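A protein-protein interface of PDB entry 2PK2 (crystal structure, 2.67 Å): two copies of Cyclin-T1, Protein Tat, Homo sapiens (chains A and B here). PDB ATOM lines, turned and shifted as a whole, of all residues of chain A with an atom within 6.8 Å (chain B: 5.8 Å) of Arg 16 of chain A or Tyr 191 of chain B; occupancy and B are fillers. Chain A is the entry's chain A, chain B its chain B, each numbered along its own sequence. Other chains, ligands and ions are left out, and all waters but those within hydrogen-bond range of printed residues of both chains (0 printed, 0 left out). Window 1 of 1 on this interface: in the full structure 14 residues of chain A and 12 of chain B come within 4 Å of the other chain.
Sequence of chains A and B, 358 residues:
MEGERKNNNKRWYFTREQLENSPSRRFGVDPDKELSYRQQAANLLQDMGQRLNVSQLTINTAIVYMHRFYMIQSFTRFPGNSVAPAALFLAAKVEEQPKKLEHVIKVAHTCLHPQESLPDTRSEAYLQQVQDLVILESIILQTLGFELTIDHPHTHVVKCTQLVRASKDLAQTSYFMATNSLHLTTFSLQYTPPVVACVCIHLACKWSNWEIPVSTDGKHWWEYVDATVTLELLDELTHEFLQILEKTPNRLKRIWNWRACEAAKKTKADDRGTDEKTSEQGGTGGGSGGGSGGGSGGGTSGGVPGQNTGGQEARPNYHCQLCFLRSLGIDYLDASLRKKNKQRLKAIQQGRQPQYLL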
ATOM      1  N   TYR A  13      -6.125  20.909  11.725  1.00  0.00           N
ATOM      2  CA  TYR A  13      -4.813  20.432  11.332  1.00  0.00           C
ATOM      3  C   TYR A  13      -3.727  21.311  11.948  1.00  0.00           C
ATOM      4  O   TYR A  13      -2.913  21.908  11.245  1.00  0.00           O
ATOM      5  CB  TYR A  13      -4.659  20.418   9.810  1.00  0.00           C
ATOM      6  CG  TYR A  13      -5.818  19.778   9.081  1.00  0.00           C
ATOM      7  CD1 TYR A  13      -6.358  18.574   9.512  1.00  0.00           C
ATOM      8  CD2 TYR A  13      -6.371  20.384   7.959  1.00  0.00           C
ATOM      9  CE1 TYR A  13      -7.417  17.985   8.849  1.00  0.00           C
ATOM     10  CE2 TYR A  13      -7.430  19.800   7.293  1.00  0.00           C
ATOM     11  CZ  TYR A  13      -7.949  18.604   7.739  1.00  0.00           C
ATOM     12  OH  TYR A  13      -9.006  18.029   7.069  1.00  0.00           O
ATOM     13  N   PHE A  14      -3.739  21.379  13.275  1.00  0.00           N
ATOM     14  CA  PHE A  14      -2.723  22.127  14.006  1.00  0.00           C
ATOM     15  C   PHE A  14      -1.333  21.606  13.664  1.00  0.00           C
ATOM     16  O   PHE A  14      -1.180  20.458  13.248  1.00  0.00           O
ATOM     17  CB  PHE A  14      -2.975  22.036  15.514  1.00  0.00           C
ATOM     18  CG  PHE A  14      -4.136  22.906  15.977  1.00  0.00           C
ATOM     19  CD1 PHE A  14      -3.902  24.098  16.638  1.00  0.00           C
ATOM     20  CD2 PHE A  14      -5.442  22.518  15.739  1.00  0.00           C
ATOM     21  CE1 PHE A  14      -4.952  24.894  17.058  1.00  0.00           C
ATOM     22  CE2 PHE A  14      -6.498  23.305  16.156  1.00  0.00           C
ATOM     23  CZ  PHE A  14      -6.254  24.496  16.816  1.00  0.00           C
ATOM     24  N   THR A  15      -0.329  22.456  13.840  1.00  0.00           N
ATOM     25  CA  THR A  15       1.057  22.056  13.633  1.00  0.00           C
ATOM     26  C   THR A  15       1.573  21.243  14.814  1.00  0.00           C
ATOM     27  O   THR A  15       0.994  21.264  15.900  1.00  0.00           O
ATOM     28  CB  THR A  15       1.958  23.289  13.440  1.00  0.00           C
ATOM     29  OG1 THR A  15       3.091  23.203  14.312  1.00  0.00           O
ATOM     30  CG2 THR A  15       1.198  24.550  13.824  1.00  0.00           C
ATOM     31  N   ARG A  16       2.674  20.523  14.615  1.00  0.00           N
ATOM     32  CA  ARG A  16       3.291  19.776  15.702  1.00  0.00           C
ATOM     33  C   ARG A  16       3.708  20.715  16.833  1.00  0.00           C
ATOM     34  O   ARG A  16       3.793  20.323  17.996  1.00  0.00           O
ATOM     35  CB  ARG A  16       4.528  19.015  15.215  1.00  0.00           C
ATOM     36  CG  ARG A  16       5.814  19.709  15.643  1.00  0.00           C
ATOM     37  CD  ARG A  16       6.822  19.780  14.516  1.00  0.00           C
ATOM     38  NE  ARG A  16       6.535  18.850  13.429  1.00  0.00           N
ATOM     39  CZ  ARG A  16       7.327  17.852  13.061  1.00  0.00           C
ATOM     40  NH1 ARG A  16       8.472  17.641  13.694  1.00  0.00           N
ATOM     41  NH2 ARG A  16       6.985  17.055  12.055  1.00  0.00           N
ATOM     42  N   GLU A  17       3.967  21.961  16.447  1.00  0.00           N
ATOM     43  CA  GLU A  17       4.327  23.006  17.394  1.00  0.00           C
ATOM     44  C   GLU A  17       3.092  23.445  18.183  1.00  0.00           C
ATOM     45  O   GLU A  17       3.184  23.704  19.381  1.00  0.00           O
ATOM     46  CB  GLU A  17       4.943  24.207  16.678  1.00  0.00           C
ATOM     47  N   GLN A  18       1.976  23.506  17.472  1.00  0.00           N
ATOM     48  CA  GLN A  18       0.693  23.963  17.978  1.00  0.00           C
ATOM     49  C   GLN A  18      -0.069  22.865  18.708  1.00  0.00           C
ATOM     50  O   GLN A  18      -1.234  23.033  19.083  1.00  0.00           O
ATOM     51  CB  GLN A  18      -0.154  24.531  16.834  1.00  0.00           C
ATOM     52  CG  GLN A  18      -0.534  25.995  17.008  1.00  0.00           C
ATOM     53  CD  GLN A  18      -1.307  26.521  15.811  1.00  0.00           C
ATOM     54  OE1 GLN A  18      -1.719  25.744  14.949  1.00  0.00           O
ATOM     55  NE2 GLN A  18      -1.502  27.833  15.760  1.00  0.00           N
ATOM     56  N   LEU A  19       0.582  21.725  18.924  1.00  0.00           N
ATOM     57  CA  LEU A  19      -0.067  20.652  19.672  1.00  0.00           C
ATOM     58  C   LEU A  19       0.678  20.404  20.980  1.00  0.00           C
ATOM     59  O   LEU A  19       0.065  20.329  22.043  1.00  0.00           O
ATOM     60  CB  LEU A  19      -0.146  19.365  18.854  1.00  0.00           C
ATOM     61  CG  LEU A  19      -1.314  18.434  19.203  1.00  0.00           C
ATOM     62  CD1 LEU A  19      -1.096  17.782  20.563  1.00  0.00           C
ATOM     63  CD2 LEU A  19      -2.632  19.201  19.169  1.00  0.00           C
ATOM     64  N   GLU A  20       1.997  20.287  20.877  1.00  0.00           N
ATOM     65  CA  GLU A  20       2.842  20.054  22.045  1.00  0.00           C
ATOM     66  C   GLU A  20       2.703  21.192  23.050  1.00  0.00           C
ATOM     67  O   GLU A  20       2.968  21.004  24.240  1.00  0.00           O
ATOM     68  CB  GLU A  20       4.295  19.869  21.611  1.00  0.00           C
ATOM     69  CG  GLU A  20       5.329  20.122  22.693  1.00  0.00           C
ATOM     70  CD  GLU A  20       5.184  19.186  23.875  1.00  0.00           C
ATOM     71  OE1 GLU A  20       4.901  17.988  23.671  1.00  0.00           O
ATOM     72  OE2 GLU A  20       5.351  19.657  25.020  1.00  0.00           O
ATOM     73  N   ASN A  21       2.280  22.362  22.589  1.00  0.00           N
ATOM     74  CA  ASN A  21       2.093  23.511  23.458  1.00  0.00           C
ATOM     75  C   ASN A  21       0.639  23.970  23.411  1.00  0.00           C
ATOM     76  O   ASN A  21       0.290  25.113  23.109  1.00  0.00           O
ATOM     77  CB  ASN A  21       3.022  24.693  23.123  1.00  0.00           C
ATOM     78  CG  ASN A  21       2.972  25.731  24.228  1.00  0.00           C
ATOM     79  OD1 ASN A  21       1.935  26.386  24.440  1.00  0.00           O
ATOM     80  ND2 ASN A  21       4.080  25.935  24.968  1.00  0.00           N
ATOM     81  N   LEU A 189      -5.833  15.652  14.169  1.00  0.00           N
ATOM     82  CA  LEU A 189      -5.490  17.068  14.190  1.00  0.00           C
ATOM     83  C   LEU A 189      -4.157  17.339  13.506  1.00  0.00           C
ATOM     84  O   LEU A 189      -3.681  18.474  13.477  1.00  0.00           O
ATOM     85  CB  LEU A 189      -5.439  17.578  15.633  1.00  0.00           C
ATOM     86  CG  LEU A 189      -6.573  17.123  16.554  1.00  0.00           C
ATOM     87  CD1 LEU A 189      -6.023  16.625  17.882  1.00  0.00           C
ATOM     88  CD2 LEU A 189      -7.573  18.248  16.769  1.00  0.00           C
ATOM     89  N   GLN A 190      -3.550  16.297  12.946  1.00  0.00           N
ATOM     90  CA  GLN A 190      -2.261  16.457  12.280  1.00  0.00           C
ATOM     91  C   GLN A 190      -2.354  16.162  10.790  1.00  0.00           C
ATOM     92  O   GLN A 190      -1.662  16.774   9.978  1.00  0.00           O
ATOM     93  CB  GLN A 190      -1.222  15.547  12.933  1.00  0.00           C
ATOM     94  CG  GLN A 190      -0.136  16.284  13.697  1.00  0.00           C
ATOM     95  CD  GLN A 190       0.797  15.329  14.419  1.00  0.00           C
ATOM     96  OE1 GLN A 190       1.673  14.715  13.808  1.00  0.00           O
ATOM     97  NE2 GLN A 190       0.608  15.203  15.728  1.00  0.00           N
ATOM     98  N   TYR A 191      -3.210  15.211  10.421  1.00  0.00           N
ATOM     99  CA  TYR A 191      -3.414  14.888   9.017  1.00  0.00           C
ATOM    100  C   TYR A 191      -4.886  14.851   8.635  1.00  0.00           C
ATOM    101  O   TYR A 191      -5.762  15.046   9.471  1.00  0.00           O
ATOM    102  CB  TYR A 191      -2.748  13.537   8.714  1.00  0.00           C
ATOM    103  CG  TYR A 191      -1.283  13.524   9.093  1.00  0.00           C
ATOM    104  CD1 TYR A 191      -0.302  13.788   8.141  1.00  0.00           C
ATOM    105  CD2 TYR A 191      -0.874  13.242  10.389  1.00  0.00           C
ATOM    106  CE1 TYR A 191       1.037  13.775   8.481  1.00  0.00           C
ATOM    107  CE2 TYR A 191       0.461  13.230  10.734  1.00  0.00           C
ATOM    108  CZ  TYR A 191       1.416  13.496   9.776  1.00  0.00           C
ATOM    109  OH  TYR A 191       2.751  13.484  10.113  1.00  0.00           O
ATOM    110  N   GLU A 236       6.718   6.615   7.953  1.00  0.00           N
ATOM    111  CA  GLU A 236       6.947   7.556   9.044  1.00  0.00           C
ATOM    112  C   GLU A 236       5.792   7.530  10.042  1.00  0.00           C
ATOM    113  O   GLU A 236       6.015   7.564  11.253  1.00  0.00           O
ATOM    114  CB  GLU A 236       7.141   8.966   8.487  1.00  0.00           C
ATOM    115  CG  GLU A 236       6.778  10.092   9.440  1.00  0.00           C
ATOM    116  CD  GLU A 236       6.411  11.382   8.728  1.00  0.00           C
ATOM    117  OE1 GLU A 236       5.564  12.143   9.241  1.00  0.00           O
ATOM    118  OE2 GLU A 236       6.987  11.614   7.644  1.00  0.00           O
ATOM    119  N   GLU A 240       5.583   5.999  13.450  1.00  0.00           N
ATOM    120  CA  GLU A 240       5.180   6.885  14.537  1.00  0.00           C
ATOM    121  C   GLU A 240       4.036   6.256  15.324  1.00  0.00           C
ATOM    122  O   GLU A 240       4.114   6.073  16.535  1.00  0.00           O
ATOM    123  CB  GLU A 240       4.766   8.247  13.994  1.00  0.00           C
ATOM    124  CG  GLU A 240       5.198   9.439  14.831  1.00  0.00           C
ATOM    125  CD  GLU A 240       5.103  10.748  14.067  1.00  0.00           C
ATOM    126  OE1 GLU A 240       5.715  10.846  12.984  1.00  0.00           O
ATOM    127  OE2 GLU A 240       4.414  11.665  14.554  1.00  0.00           O
ATOM    128  N   TYR B  13       2.420  28.425   7.561  1.00  0.00           N
ATOM    129  CA  TYR B  13       2.603  27.110   8.149  1.00  0.00           C
ATOM    130  C   TYR B  13       1.494  26.195   7.627  1.00  0.00           C
ATOM    131  O   TYR B  13       0.308  26.461   7.819  1.00  0.00           O
ATOM    132  CB  TYR B  13       2.598  27.156   9.673  1.00  0.00           C
ATOM    133  CG  TYR B  13       3.564  28.150  10.274  1.00  0.00           C
ATOM    134  CD1 TYR B  13       4.912  28.132   9.940  1.00  0.00           C
ATOM    135  CD2 TYR B  13       3.127  29.110  11.180  1.00  0.00           C
ATOM    136  CE1 TYR B  13       5.795  29.042  10.492  1.00  0.00           C
ATOM    137  CE2 TYR B  13       4.003  30.023  11.735  1.00  0.00           C
ATOM    138  CZ  TYR B  13       5.337  29.984  11.388  1.00  0.00           C
ATOM    139  OH  TYR B  13       6.213  30.892  11.938  1.00  0.00           O
ATOM    140  N   THR B 186      13.228  23.148   3.737  1.00  0.00           N
ATOM    141  CA  THR B 186      12.122  24.100   3.691  1.00  0.00           C
ATOM    142  C   THR B 186      11.542  24.324   5.088  1.00  0.00           C
ATOM    143  O   THR B 186      10.333  24.472   5.263  1.00  0.00           O
ATOM    144  CB  THR B 186      10.999  23.628   2.754  1.00  0.00           C
ATOM    145  OG1 THR B 186      10.067  22.825   3.491  1.00  0.00           O
ATOM    146  CG2 THR B 186      11.563  22.747   1.650  1.00  0.00           C
ATOM    147  N   PHE B 187      12.428  24.346   6.075  1.00  0.00           N
ATOM    148  CA  PHE B 187      12.042  24.491   7.475  1.00  0.00           C
ATOM    149  C   PHE B 187      11.365  25.828   7.740  1.00  0.00           C
ATOM    150  O   PHE B 187      10.696  25.996   8.764  1.00  0.00           O
ATOM    151  CB  PHE B 187      13.271  24.326   8.375  1.00  0.00           C
ATOM    152  CG  PHE B 187      13.686  22.876   8.569  1.00  0.00           C
ATOM    153  CD1 PHE B 187      12.745  21.863   8.548  1.00  0.00           C
ATOM    154  CD2 PHE B 187      15.015  22.542   8.763  1.00  0.00           C
ATOM    155  CE1 PHE B 187      13.122  20.542   8.715  1.00  0.00           C
ATOM    156  CE2 PHE B 187      15.403  21.226   8.930  1.00  0.00           C
ATOM    157  CZ  PHE B 187      14.453  20.222   8.904  1.00  0.00           C
ATOM    158  N   SER B 188      11.525  26.777   6.826  1.00  0.00           N
ATOM    159  CA  SER B 188      10.937  28.103   6.959  1.00  0.00           C
ATOM    160  C   SER B 188       9.413  28.039   6.934  1.00  0.00           C
ATOM    161  O   SER B 188       8.733  28.838   7.583  1.00  0.00           O
ATOM    162  CB  SER B 188      11.448  29.027   5.852  1.00  0.00           C
ATOM    163  OG  SER B 188      10.535  30.073   5.570  1.00  0.00           O
ATOM    164  N   LEU B 189       8.877  27.090   6.174  1.00  0.00           N
ATOM    165  CA  LEU B 189       7.434  26.957   6.018  1.00  0.00           C
ATOM    166  C   LEU B 189       6.879  25.819   6.865  1.00  0.00           C
ATOM    167  O   LEU B 189       5.686  25.517   6.817  1.00  0.00           O
ATOM    168  CB  LEU B 189       7.071  26.728   4.548  1.00  0.00           C
ATOM    169  CG  LEU B 189       7.813  27.591   3.525  1.00  0.00           C
ATOM    170  CD1 LEU B 189       8.297  26.725   2.371  1.00  0.00           C
ATOM    171  CD2 LEU B 189       6.941  28.729   3.019  1.00  0.00           C
ATOM    172  N   GLN B 190       7.741  25.173   7.640  1.00  0.00           N
ATOM    173  CA  GLN B 190       7.321  24.021   8.429  1.00  0.00           C
ATOM    174  C   GLN B 190       7.432  24.285   9.924  1.00  0.00           C
ATOM    175  O   GLN B 190       6.629  23.789  10.715  1.00  0.00           O
ATOM    176  CB  GLN B 190       8.159  22.799   8.047  1.00  0.00           C
ATOM    177  CG  GLN B 190       7.378  21.712   7.322  1.00  0.00           C
ATOM    178  CD  GLN B 190       8.214  20.468   7.095  1.00  0.00           C
ATOM    179  OE1 GLN B 190       8.418  19.674   8.015  1.00  0.00           O
ATOM    180  NE2 GLN B 190       8.693  20.303   5.868  1.00  0.00           N
ATOM    181  N   TYR B 191       8.433  25.065  10.320  1.00  0.00           N
ATOM    182  CA  TYR B 191       8.657  25.334  11.734  1.00  0.00           C
ATOM    183  C   TYR B 191       8.821  26.822  12.022  1.00  0.00           C
ATOM    184  O   TYR B 191       8.799  27.652  11.111  1.00  0.00           O
ATOM    185  CB  TYR B 191       9.899  24.566  12.202  1.00  0.00           C
ATOM    186  CG  TYR B 191       9.811  23.085  11.900  1.00  0.00           C
ATOM    187  CD1 TYR B 191       9.372  22.193  12.871  1.00  0.00           C
ATOM    188  CD2 TYR B 191      10.164  22.576  10.658  1.00  0.00           C
ATOM    189  CE1 TYR B 191       9.290  20.837  12.604  1.00  0.00           C
ATOM    190  CE2 TYR B 191      10.082  21.227  10.385  1.00  0.00           C
ATOM    191  CZ  TYR B 191       9.644  20.359  11.362  1.00  0.00           C
ATOM    192  OH  TYR B 191       9.560  19.010  11.101  1.00  0.00           O
ATOM    193  N   THR B 192       8.976  27.137  13.304  1.00  0.00           N
ATOM    194  CA  THR B 192       9.157  28.512  13.753  1.00  0.00           C
ATOM    195  C   THR B 192      10.624  28.795  14.068  1.00  0.00           C
ATOM    196  O   THR B 192      11.338  27.889  14.489  1.00  0.00           O
ATOM    197  CB  THR B 192       8.311  28.822  14.999  1.00  0.00           C
ATOM    198  OG1 THR B 192       8.997  28.358  16.169  1.00  0.00           O
ATOM    199  CG2 THR B 192       6.993  28.064  14.943  1.00  0.00           C
ATOM    200  N   PRO B 193      11.040  30.035  13.842  1.00  0.00           N
ATOM    201  CA  PRO B 193      12.406  30.464  14.170  1.00  0.00           C
ATOM    202  C   PRO B 193      12.836  30.059  15.574  1.00  0.00           C
ATOM    203  O   PRO B 193      13.958  29.554  15.728  1.00  0.00           O
ATOM    204  CB  PRO B 193      12.324  31.985  14.041  1.00  0.00           C
ATOM    205  CG  PRO B 193      11.253  32.216  13.029  1.00  0.00           C
ATOM    206  CD  PRO B 193      10.247  31.114  13.225  1.00  0.00           C
ATOM    207  N   VAL B 195      11.959  27.570  17.010  1.00  0.00           N
ATOM    208  CA  VAL B 195      11.945  26.111  17.014  1.00  0.00           C
ATOM    209  C   VAL B 195      12.861  25.548  15.933  1.00  0.00           C
ATOM    210  O   VAL B 195      13.072  24.340  15.851  1.00  0.00           O
ATOM    211  CB  VAL B 195      10.525  25.555  16.818  1.00  0.00           C
ATOM    212  CG1 VAL B 195      10.511  24.039  16.939  1.00  0.00           C
ATOM    213  CG2 VAL B 195       9.565  26.174  17.825  1.00  0.00           C
ATOM    214  N   VAL B 196      13.415  26.425  15.100  1.00  0.00           N
ATOM    215  CA  VAL B 196      14.367  25.995  14.081  1.00  0.00           C
ATOM    216  C   VAL B 196      15.796  26.113  14.609  1.00  0.00           C
ATOM    217  O   VAL B 196      16.634  25.251  14.357  1.00  0.00           O
ATOM    218  CB  VAL B 196      14.248  26.809  12.783  1.00  0.00           C
ATOM    219  CG1 VAL B 196      15.116  26.198  11.689  1.00  0.00           C
ATOM    220  CG2 VAL B 196      12.802  26.889  12.323  1.00  0.00           C
ATOM    221  N   LEU B 233      11.570  15.708  19.498  1.00  0.00           N
ATOM    222  CA  LEU B 233      11.444  16.484  18.277  1.00  0.00           C
ATOM    223  C   LEU B 233      12.791  17.057  17.857  1.00  0.00           C
ATOM    224  O   LEU B 233      13.103  17.150  16.673  1.00  0.00           O
ATOM    225  CB  LEU B 233      10.428  17.611  18.464  1.00  0.00           C
ATOM    226  CG  LEU B 233      10.124  18.472  17.234  1.00  0.00           C
ATOM    227  CD1 LEU B 233       8.683  18.284  16.790  1.00  0.00           C
ATOM    228  CD2 LEU B 233      10.419  19.931  17.534  1.00  0.00           C
ATOM    229  N   GLU B 236      14.231  14.194  16.542  1.00  0.00           N
ATOM    230  CA  GLU B 236      13.263  13.853  15.516  1.00  0.00           C
ATOM    231  C   GLU B 236      13.498  14.648  14.242  1.00  0.00           C
ATOM    232  O   GLU B 236      13.419  14.136  13.131  1.00  0.00           O
ATOM    233  CB  GLU B 236      11.844  14.102  16.031  1.00  0.00           C
ATOM    234  CG  GLU B 236      10.817  14.129  14.914  1.00  0.00           C
ATOM    235  CD  GLU B 236       9.402  14.217  15.447  1.00  0.00           C
ATOM    236  OE1 GLU B 236       8.525  14.710  14.705  1.00  0.00           O
ATOM    237  OE2 GLU B 236       9.138  13.804  16.599  1.00  0.00           O
ATOM    238  N   LEU B 237      13.806  15.930  14.391  1.00  0.00           N
ATOM    239  CA  LEU B 237      14.085  16.840  13.305  1.00  0.00           C
ATOM    240  C   LEU B 237      15.514  16.722  12.796  1.00  0.00           C
ATOM    241  O   LEU B 237      15.781  16.904  11.618  1.00  0.00           O
ATOM    242  CB  LEU B 237      13.816  18.271  13.803  1.00  0.00           C
ATOM    243  CG  LEU B 237      12.381  18.487  14.315  1.00  0.00           C
ATOM    244  CD1 LEU B 237      12.159  19.928  14.730  1.00  0.00           C
ATOM    245  CD2 LEU B 237      11.396  18.064  13.235  1.00  0.00           C
ATOM    246  N   GLU B 240      15.745  14.226   9.961  1.00  0.00           N
ATOM    247  CA  GLU B 240      15.300  14.830   8.700  1.00  0.00           C
ATOM    248  C   GLU B 240      16.359  15.814   8.202  1.00  0.00           C
ATOM    249  O   GLU B 240      16.850  15.694   7.081  1.00  0.00           O
ATOM    250  CB  GLU B 240      13.958  15.531   8.872  1.00  0.00           C
ATOM    251  CG  GLU B 240      13.004  15.348   7.699  1.00  0.00           C
ATOM    252  CD  GLU B 240      11.806  16.279   7.777  1.00  0.00           C
ATOM    253  OE1 GLU B 240      12.034  17.505   7.829  1.00  0.00           O
ATOM    254  OE2 GLU B 240      10.658  15.791   7.791  1.00  0.00           O
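NH1 of Arg 16 of chain A lies within salt-bridge range of OE1 of Glu 236 of chain B, at 3.1 Å. The guanidinium group of Arg 16 of chain A is in hydrogen-bond range of the side-chain hydroxyl of Tyr 191 of chain B.
The side-chain amide oxygen of Gln 190 of chain B sits close to the side-chain hydroxyl of Tyr 191 of chain B, at 3.4 Å.
Arg 16 of chain A touches Leu 233 of chain B (NH1 to CD1, 3.2 Å). Leu 237 of chain B touches Arg 16 of chain A.
Arg 16 of chain A touches four residues of chain B. Of chain A, only Arg 16 (3.1 Å) comes within 4 Å of Tyr 191 of chain B. Of the printed residues of chain A, Leu 237 of chain B touches Arg 16. Of the printed residues of chain A, Leu 233 of chain B touches Arg 16. Asn 21 of chain A touches none of the printed residues of chain B. The nearest residue of chain A that does not touch Tyr 191 of chain B is Glu 17 of chain A (6.2 Å). The nearest printed residue of chain A that does not touch Leu 237 of chain B is Glu 17 of chain A (8.6 Å).
Of the 15 printed residues of chain B, 4 touch a printed residue of chain A. Among the printed residues, 4 pairs touch across the chains. Among the printed residues, Asp or Glu carboxylates within 4 Å of a Lys or Arg side-chain nitrogen of the other chain: Arg 16 of chain A with Glu 236 of chain B (3.1 Å).
Positions printed for both chains: 13, 189, 190, 191, 236 and 240. Of the 4 pairs that touch across the chains among the printed residues, none has its exchanged pair printed and touching as well.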
